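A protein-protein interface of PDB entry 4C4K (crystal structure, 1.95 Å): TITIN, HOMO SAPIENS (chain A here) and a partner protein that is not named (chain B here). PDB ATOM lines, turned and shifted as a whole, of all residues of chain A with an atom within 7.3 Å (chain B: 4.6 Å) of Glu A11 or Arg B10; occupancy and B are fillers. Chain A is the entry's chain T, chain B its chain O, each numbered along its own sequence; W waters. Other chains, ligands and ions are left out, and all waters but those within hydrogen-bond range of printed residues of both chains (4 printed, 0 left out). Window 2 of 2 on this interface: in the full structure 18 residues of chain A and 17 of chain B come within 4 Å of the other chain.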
ATOM      1  N   LYS A   9       9.898  23.373  -4.940  1.00  0.00           N
ATOM      2  CA  LYS A   9       9.765  22.185  -4.120  1.00  0.00           C
ATOM      3  C   LYS A   9      10.225  22.492  -2.699  1.00  0.00           C
ATOM      4  O   LYS A   9      11.348  22.944  -2.499  1.00  0.00           O
ATOM      5  CB  LYS A   9      10.585  21.024  -4.704  1.00  0.00           C
ATOM      6  CG  LYS A   9      10.184  19.648  -4.186  1.00  0.00           C
ATOM      7  CD  LYS A   9      10.978  18.554  -4.898  1.00  0.00           C
ATOM      8  CE  LYS A   9      11.488  17.478  -3.966  1.00  0.00           C
ATOM      9  NZ  LYS A   9      12.574  17.966  -3.065  1.00  0.00           N
ATOM     10  N   ILE A  10       9.365  22.213  -1.726  1.00  0.00           N
ATOM     11  CA  ILE A  10       9.682  22.343  -0.295  1.00  0.00           C
ATOM     12  C   ILE A  10      10.546  21.105   0.026  1.00  0.00           C
ATOM     13  O   ILE A  10      10.133  19.979  -0.290  1.00  0.00           O
ATOM     14  CB  ILE A  10       8.374  22.357   0.536  1.00  0.00           C
ATOM     15  CG1 ILE A  10       7.564  23.613   0.251  1.00  0.00           C
ATOM     16  CG2 ILE A  10       8.672  22.175   2.060  1.00  0.00           C
ATOM     17  CD1 ILE A  10       6.172  23.634   0.756  1.00  0.00           C
ATOM     18  N   GLU A  11      11.742  21.304   0.601  1.00  0.00           N
ATOM     19  CA  GLU A  11      12.627  20.173   0.944  1.00  0.00           C
ATOM     20  C   GLU A  11      11.914  19.203   1.901  1.00  0.00           C
ATOM     21  O   GLU A  11      11.744  18.035   1.571  1.00  0.00           O
ATOM     22  CB  GLU A  11      13.955  20.673   1.567  1.00  0.00           C
ATOM     23  CG  GLU A  11      14.824  19.611   2.239  1.00  0.00           C
ATOM     24  CD  GLU A  11      15.342  18.497   1.348  1.00  0.00           C
ATOM     25  OE1 GLU A  11      15.701  18.777   0.181  1.00  0.00           O
ATOM     26  OE2 GLU A  11      15.375  17.335   1.814  1.00  0.00           O
ATOM     27  N   ALA A  12      11.507  19.701   3.081  1.00  0.00           N
ATOM     28  CA  ALA A  12      10.884  18.921   4.147  1.00  0.00           C
ATOM     29  C   ALA A  12      10.335  19.871   5.223  1.00  0.00           C
ATOM     30  O   ALA A  12      10.987  20.843   5.598  1.00  0.00           O
ATOM     31  CB  ALA A  12      11.918  17.973   4.762  1.00  0.00           C
ATOM     32  N   LEU A  13       9.136  19.599   5.703  1.00  0.00           N
ATOM     33  CA  LEU A  13       8.534  20.368   6.771  1.00  0.00           C
ATOM     34  C   LEU A  13       7.950  19.357   7.756  1.00  0.00           C
ATOM     35  O   LEU A  13       7.247  18.436   7.320  1.00  0.00           O
ATOM     36  CB  LEU A  13       7.445  21.340   6.241  1.00  0.00           C
ATOM     37  CG  LEU A  13       6.851  22.324   7.270  1.00  0.00           C
ATOM     38  CD1 LEU A  13       7.891  23.342   7.731  1.00  0.00           C
ATOM     39  CD2 LEU A  13       5.653  23.087   6.677  1.00  0.00           C
ATOM     40  N   ALA A  28      12.564  26.243  10.398  1.00  0.00           N
ATOM     41  CA  ALA A  28      13.259  26.593   9.164  1.00  0.00           C
ATOM     42  C   ALA A  28      12.970  25.542   8.105  1.00  0.00           C
ATOM     43  O   ALA A  28      12.852  24.353   8.411  1.00  0.00           O
ATOM     44  CB  ALA A  28      14.747  26.732   9.420  1.00  0.00           C
ATOM     45  N   CYS A  29      12.786  25.990   6.866  1.00  0.00           N
ATOM     46  CA  CYS A  29      12.450  25.102   5.757  1.00  0.00           C
ATOM     47  C   CYS A  29      13.186  25.487   4.471  1.00  0.00           C
ATOM     48  O   CYS A  29      13.099  26.624   4.023  1.00  0.00           O
ATOM     49  CB  CYS A  29      10.933  25.064   5.552  1.00  0.00           C
ATOM     50  SG  CYS A  29      10.388  23.811   4.363  1.00  0.00           S
ATOM     51  N   ALA A  30      13.928  24.544   3.901  1.00  0.00           N
ATOM     52  CA  ALA A  30      14.661  24.749   2.649  1.00  0.00           C
ATOM     53  C   ALA A  30      13.724  24.548   1.471  1.00  0.00           C
ATOM     54  O   ALA A  30      12.703  23.841   1.576  1.00  0.00           O
ATOM     55  CB  ALA A  30      15.834  23.779   2.545  1.00  0.00           C
ATOM     56  N   PHE A  31      14.086  25.146   0.336  1.00  0.00           N
ATOM     57  CA  PHE A  31      13.328  24.984  -0.890  1.00  0.00           C
ATOM     58  C   PHE A  31      14.194  25.178  -2.123  1.00  0.00           C
ATOM     59  O   PHE A  31      15.280  25.756  -2.043  1.00  0.00           O
ATOM     60  CB  PHE A  31      12.098  25.914  -0.932  1.00  0.00           C
ATOM     61  CG  PHE A  31      12.393  27.390  -0.786  1.00  0.00           C
ATOM     62  CD1 PHE A  31      12.690  28.173  -1.901  1.00  0.00           C
ATOM     63  CD2 PHE A  31      12.361  27.999   0.461  1.00  0.00           C
ATOM     64  CE1 PHE A  31      12.994  29.535  -1.759  1.00  0.00           C
ATOM     65  CE2 PHE A  31      12.690  29.350   0.606  1.00  0.00           C
ATOM     66  CZ  PHE A  31      12.986  30.115  -0.504  1.00  0.00           C
ATOM     67  N   THR A  32      13.699  24.696  -3.259  1.00  0.00           N
ATOM     68  CA  THR A  32      14.327  24.869  -4.564  1.00  0.00           C
ATOM     69  C   THR A  32      13.268  25.396  -5.529  1.00  0.00           C
ATOM     70  O   THR A  32      12.083  25.392  -5.209  1.00  0.00           O
ATOM     71  CB  THR A  32      14.986  23.571  -5.059  1.00  0.00           C
ATOM     72  OG1 THR A  32      14.005  22.541  -5.093  1.00  0.00           O
ATOM     73  CG2 THR A  32      16.183  23.158  -4.212  1.00  0.00           C
ATOM     74  N   ASP A  63      17.079  30.209  -0.581  1.00  0.00           N
ATOM     75  CA  ASP A  63      16.749  28.773  -0.480  1.00  0.00           C
ATOM     76  C   ASP A  63      16.300  28.313   0.911  1.00  0.00           C
ATOM     77  O   ASP A  63      16.257  27.114   1.183  1.00  0.00           O
ATOM     78  CB  ASP A  63      17.933  27.915  -1.003  1.00  0.00           C
ATOM     79  CG  ASP A  63      19.253  28.104  -0.261  1.00  0.00           C
ATOM     80  OD1 ASP A  63      19.246  28.724   0.831  1.00  0.00           O
ATOM     81  OD2 ASP A  63      20.293  27.630  -0.770  1.00  0.00           O
ATOM     82  N   LEU A  64      16.018  29.260   1.798  1.00  0.00           N
ATOM     83  CA  LEU A  64      15.578  28.965   3.150  1.00  0.00           C
ATOM     84  C   LEU A  64      14.577  30.013   3.648  1.00  0.00           C
ATOM     85  O   LEU A  64      14.777  31.220   3.468  1.00  0.00           O
ATOM     86  CB  LEU A  64      16.790  28.868   4.110  1.00  0.00           C
ATOM     87  CG  LEU A  64      16.508  28.442   5.552  1.00  0.00           C
ATOM     88  CD1 LEU A  64      16.265  26.937   5.666  1.00  0.00           C
ATOM     89  CD2 LEU A  64      17.655  28.816   6.459  1.00  0.00           C
ATOM     90  N   LEU A  82       3.126  26.604   4.594  1.00  0.00           N
ATOM     91  CA  LEU A  82       4.132  27.222   3.764  1.00  0.00           C
ATOM     92  C   LEU A  82       3.751  26.952   2.293  1.00  0.00           C
ATOM     93  O   LEU A  82       3.601  25.804   1.890  1.00  0.00           O
ATOM     94  CB  LEU A  82       5.545  26.656   4.080  1.00  0.00           C
ATOM     95  CG  LEU A  82       6.650  27.054   3.094  1.00  0.00           C
ATOM     96  CD1 LEU A  82       6.826  28.592   3.015  1.00  0.00           C
ATOM     97  CD2 LEU A  82       7.976  26.317   3.408  1.00  0.00           C
ATOM     98  N   LEU A  84       4.826  27.880  -1.888  1.00  0.00           N
ATOM     99  CA  LEU A  84       5.812  28.406  -2.806  1.00  0.00           C
ATOM    100  C   LEU A  84       5.192  28.429  -4.182  1.00  0.00           C
ATOM    101  O   LEU A  84       4.436  27.526  -4.527  1.00  0.00           O
ATOM    102  CB  LEU A  84       7.040  27.494  -2.874  1.00  0.00           C
ATOM    103  CG  LEU A  84       7.721  27.090  -1.600  1.00  0.00           C
ATOM    104  CD1 LEU A  84       8.872  26.146  -1.953  1.00  0.00           C
ATOM    105  CD2 LEU A  84       8.202  28.294  -0.819  1.00  0.00           C
ATOM    106  N   ASP A  91       4.137  24.538  -4.656  1.00  0.00           N
ATOM    107  CA  ASP A  91       4.293  23.493  -3.665  1.00  0.00           C
ATOM    108  C   ASP A  91       3.778  24.064  -2.380  1.00  0.00           C
ATOM    109  O   ASP A  91       3.819  25.287  -2.182  1.00  0.00           O
ATOM    110  CB  ASP A  91       5.745  23.014  -3.531  1.00  0.00           C
ATOM    111  CG  ASP A  91       5.863  21.653  -2.853  1.00  0.00           C
ATOM    112  OD1 ASP A  91       4.833  20.932  -2.758  1.00  0.00           O
ATOM    113  OD2 ASP A  91       6.960  21.321  -2.395  1.00  0.00           O
ATOM    114  N   THR B   9      22.422  27.797   8.483  1.00  0.00           N
ATOM    115  CA  THR B   9      22.283  27.240   7.124  1.00  0.00           C
ATOM    116  C   THR B   9      21.232  26.115   7.079  1.00  0.00           C
ATOM    117  O   THR B   9      20.968  25.472   8.082  1.00  0.00           O
ATOM    118  CB  THR B   9      23.641  26.774   6.542  1.00  0.00           C
ATOM    119  OG1 THR B   9      24.270  25.844   7.424  1.00  0.00           O
ATOM    120  CG2 THR B   9      24.579  27.925   6.206  1.00  0.00           C
ATOM    121  N   ARG B  10      20.652  25.870   5.916  1.00  0.00           N
ATOM    122  CA  ARG B  10      19.662  24.815   5.722  1.00  0.00           C
ATOM    123  C   ARG B  10      20.222  23.428   6.100  1.00  0.00           C
ATOM    124  O   ARG B  10      21.400  23.167   5.816  1.00  0.00           O
ATOM    125  CB  ARG B  10      19.132  24.820   4.269  1.00  0.00           C
ATOM    126  CG  ARG B  10      20.185  24.923   3.171  1.00  0.00           C
ATOM    127  CD  ARG B  10      19.772  24.159   1.913  1.00  0.00           C
ATOM    128  NE  ARG B  10      19.363  22.788   2.231  1.00  0.00           N
ATOM    129  CZ  ARG B  10      18.685  21.985   1.418  1.00  0.00           C
ATOM    130  NH1 ARG B  10      18.323  22.402   0.209  1.00  0.00           N
ATOM    131  NH2 ARG B  10      18.341  20.767   1.816  1.00  0.00           N
ATOM    132  N   PRO B  11      19.428  22.532   6.755  1.00  0.00           N
ATOM    133  CA  PRO B  11      19.954  21.181   7.043  1.00  0.00           C
ATOM    134  C   PRO B  11      20.176  20.476   5.718  1.00  0.00           C
ATOM    135  O   PRO B  11      19.427  20.704   4.763  1.00  0.00           O
ATOM    136  CB  PRO B  11      18.844  20.515   7.859  1.00  0.00           C
ATOM    137  CG  PRO B  11      17.598  21.265   7.487  1.00  0.00           C
ATOM    138  CD  PRO B  11      18.004  22.661   7.137  1.00  0.00           C
ATOM    139  N   LYS B  12      21.261  19.720   5.610  1.00  0.00           N
ATOM    140  CA  LYS B  12      21.554  19.099   4.324  1.00  0.00           C
ATOM    141  C   LYS B  12      21.796  17.615   4.463  1.00  0.00           C
ATOM    142  O   LYS B  12      22.442  17.201   5.422  1.00  0.00           O
ATOM    143  CB  LYS B  12      22.781  19.768   3.700  1.00  0.00           C
ATOM    144  CG  LYS B  12      22.580  21.229   3.294  1.00  0.00           C
ATOM    145  CD  LYS B  12      23.902  21.956   3.082  1.00  0.00           C
ATOM    146  CE  LYS B  12      23.661  23.404   2.745  1.00  0.00           C
ATOM    147  NZ  LYS B  12      24.763  24.275   3.225  1.00  0.00           N
ATOM    148  N   SER B  25      23.894  17.217   8.035  1.00  0.00           N
ATOM    149  CA  SER B  25      24.534  18.251   8.846  1.00  0.00           C
ATOM    150  C   SER B  25      23.830  19.591   8.771  1.00  0.00           C
ATOM    151  O   SER B  25      23.101  19.876   7.809  1.00  0.00           O
ATOM    152  CB  SER B  25      26.000  18.428   8.440  1.00  0.00           C
ATOM    153  OG  SER B  25      26.059  18.994   7.147  1.00  0.00           O
ATOM    154  N   CYS B  26      24.063  20.410   9.797  1.00  0.00           N
ATOM    155  CA  CYS B  26      23.594  21.790   9.873  1.00  0.00           C
ATOM    156  C   CYS B  26      24.390  22.606  10.868  1.00  0.00           C
ATOM    157  O   CYS B  26      25.042  22.064  11.754  1.00  0.00           O
ATOM    158  CB  CYS B  26      22.102  21.872  10.149  1.00  0.00           C
ATOM    159  SG  CYS B  26      21.592  20.925  11.582  1.00  0.00           S
ATOM    160  N   ALA B  89      13.768  20.213   9.046  1.00  0.00           N
ATOM    161  CA  ALA B  89      13.746  18.839   8.593  1.00  0.00           C
ATOM    162  C   ALA B  89      14.470  18.681   7.276  1.00  0.00           C
ATOM    163  O   ALA B  89      14.718  19.656   6.573  1.00  0.00           O
ATOM    164  CB  ALA B  89      12.305  18.351   8.479  1.00  0.00           C
ATOM    165  N   VAL B  90      14.851  17.457   6.977  1.00  0.00           N
ATOM    166  CA  VAL B  90      15.535  17.091   5.728  1.00  0.00           C
ATOM    167  C   VAL B  90      15.107  15.660   5.397  1.00  0.00           C
ATOM    168  O   VAL B  90      14.917  14.842   6.308  1.00  0.00           O
ATOM    169  CB  VAL B  90      17.089  17.263   5.843  1.00  0.00           C
ATOM    170  CG1 VAL B  90      17.713  16.245   6.813  1.00  0.00           C
ATOM    171  CG2 VAL B  90      17.773  17.218   4.464  1.00  0.00           C
ATOM    172  N   GLY B  91      14.922  15.393   4.113  1.00  0.00           N
ATOM    173  CA  GLY B  91      14.529  14.088   3.596  1.00  0.00           C
ATOM    174  C   GLY B  91      15.730  13.290   3.129  1.00  0.00           C
ATOM    175  O   GLY B  91      16.748  13.848   2.699  1.00  0.00           O
HETATM  176  O   HOH W   1      17.411  15.841   1.006  1.00  0.00           O
HETATM  177  O   HOH W   2      14.342  21.917   5.015  1.00  0.00           O
HETATM  178  O   HOH W   3      11.706  21.965   8.093  1.00  0.00           O
HETATM  179  O   HOH W   4      16.045  21.157  -1.115  1.00  0.00           O
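Water W1 bridges the side-chain carboxylate (OE2) of Glu A11 and the backbone carbonyl oxygen (O) of Gly B91. Water W3 lies within hydrogen-bond range of the backbone carbonyl oxygen (O) of Ala A28 (2.7 Å), the backbone carbonyl oxygen (O) of Ala A12 (2.8 Å) and the backbone NH (N) of Ala B89 (2.9 Å). Water W4 lies within hydrogen-bond range of OE1 of Glu A11 (2.7 Å) and NH1 of Arg B10 (2.9 Å). Water W2 bridges the backbone carbonyl oxygen (O) of Ala B89 and the backbone NH (N) of Ala A30.
Printed residues of chain B that touch a printed residue of chain A: Arg B10, Ala B89, Val B90 and Gly B91. Printed residues of chain A that touch a printed residue of chain B: Glu A11, Ala A12, Ala A30 and Leu A64. Among the printed residues, 7 pairs touch across the chains.
The backbone NH of Gly B91 is in hydrogen-bond range of the side-chain carboxylate of Glu A11 (3.0 Å). NH2 of Arg B10 lies within salt-bridge range of OE1 of Glu A11 (3.7 Å).
N of Glu A11 is in hydrogen-bond range of O of Ala A30, 2.9 Å away. The backbone carbonyl oxygen (O) of Ala A12 lies within hydrogen-bond range of the side-chain sulfur (SG) of Cys A29 (3.3 Å).
Of chain B, only Arg B10 (3.7 Å), Val B90 (3.6 Å) and Gly B91 (3.0 Å) come within 4 Å of Glu A11. Printed residues of chain B within 4 Å of Ala A12: Ala B89 and Val B90. Printed residues of chain B within 4 Å of Ala A30: Arg B10. Thr A32 touches none of the printed residues of chain B. Of the printed residues of chain B, Leu A64 touches Arg B10 (3.8 Å). Of the printed residues of chain A, Arg B10 touches Glu A11 (3.7 Å), Ala A30 (3.6 Å) and Leu A64 (3.8 Å). Pro B11 touches none of the printed residues of chain A. Printed residues of chain A within 4 Å of Ala B89: Ala A12 (3.7 Å). Printed residues of chain A within 4 Å of Val B90: Glu A11 (3.6 Å) and Ala A12 (3.7 Å). The nearest printed residue of chain A that does not touch Val B90 is Leu A13 (6.2 Å).
Among the printed residues, pairs that only touch across the chains: Ala A30 with Arg B10 (3.6 Å), Glu A11 with Val B90 (3.6 Å), Ala A12 with Ala B89 (3.7 Å), Ala A12 with Val B90 (3.7 Å) and Leu A64 with Arg B10 (3.8 Å).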
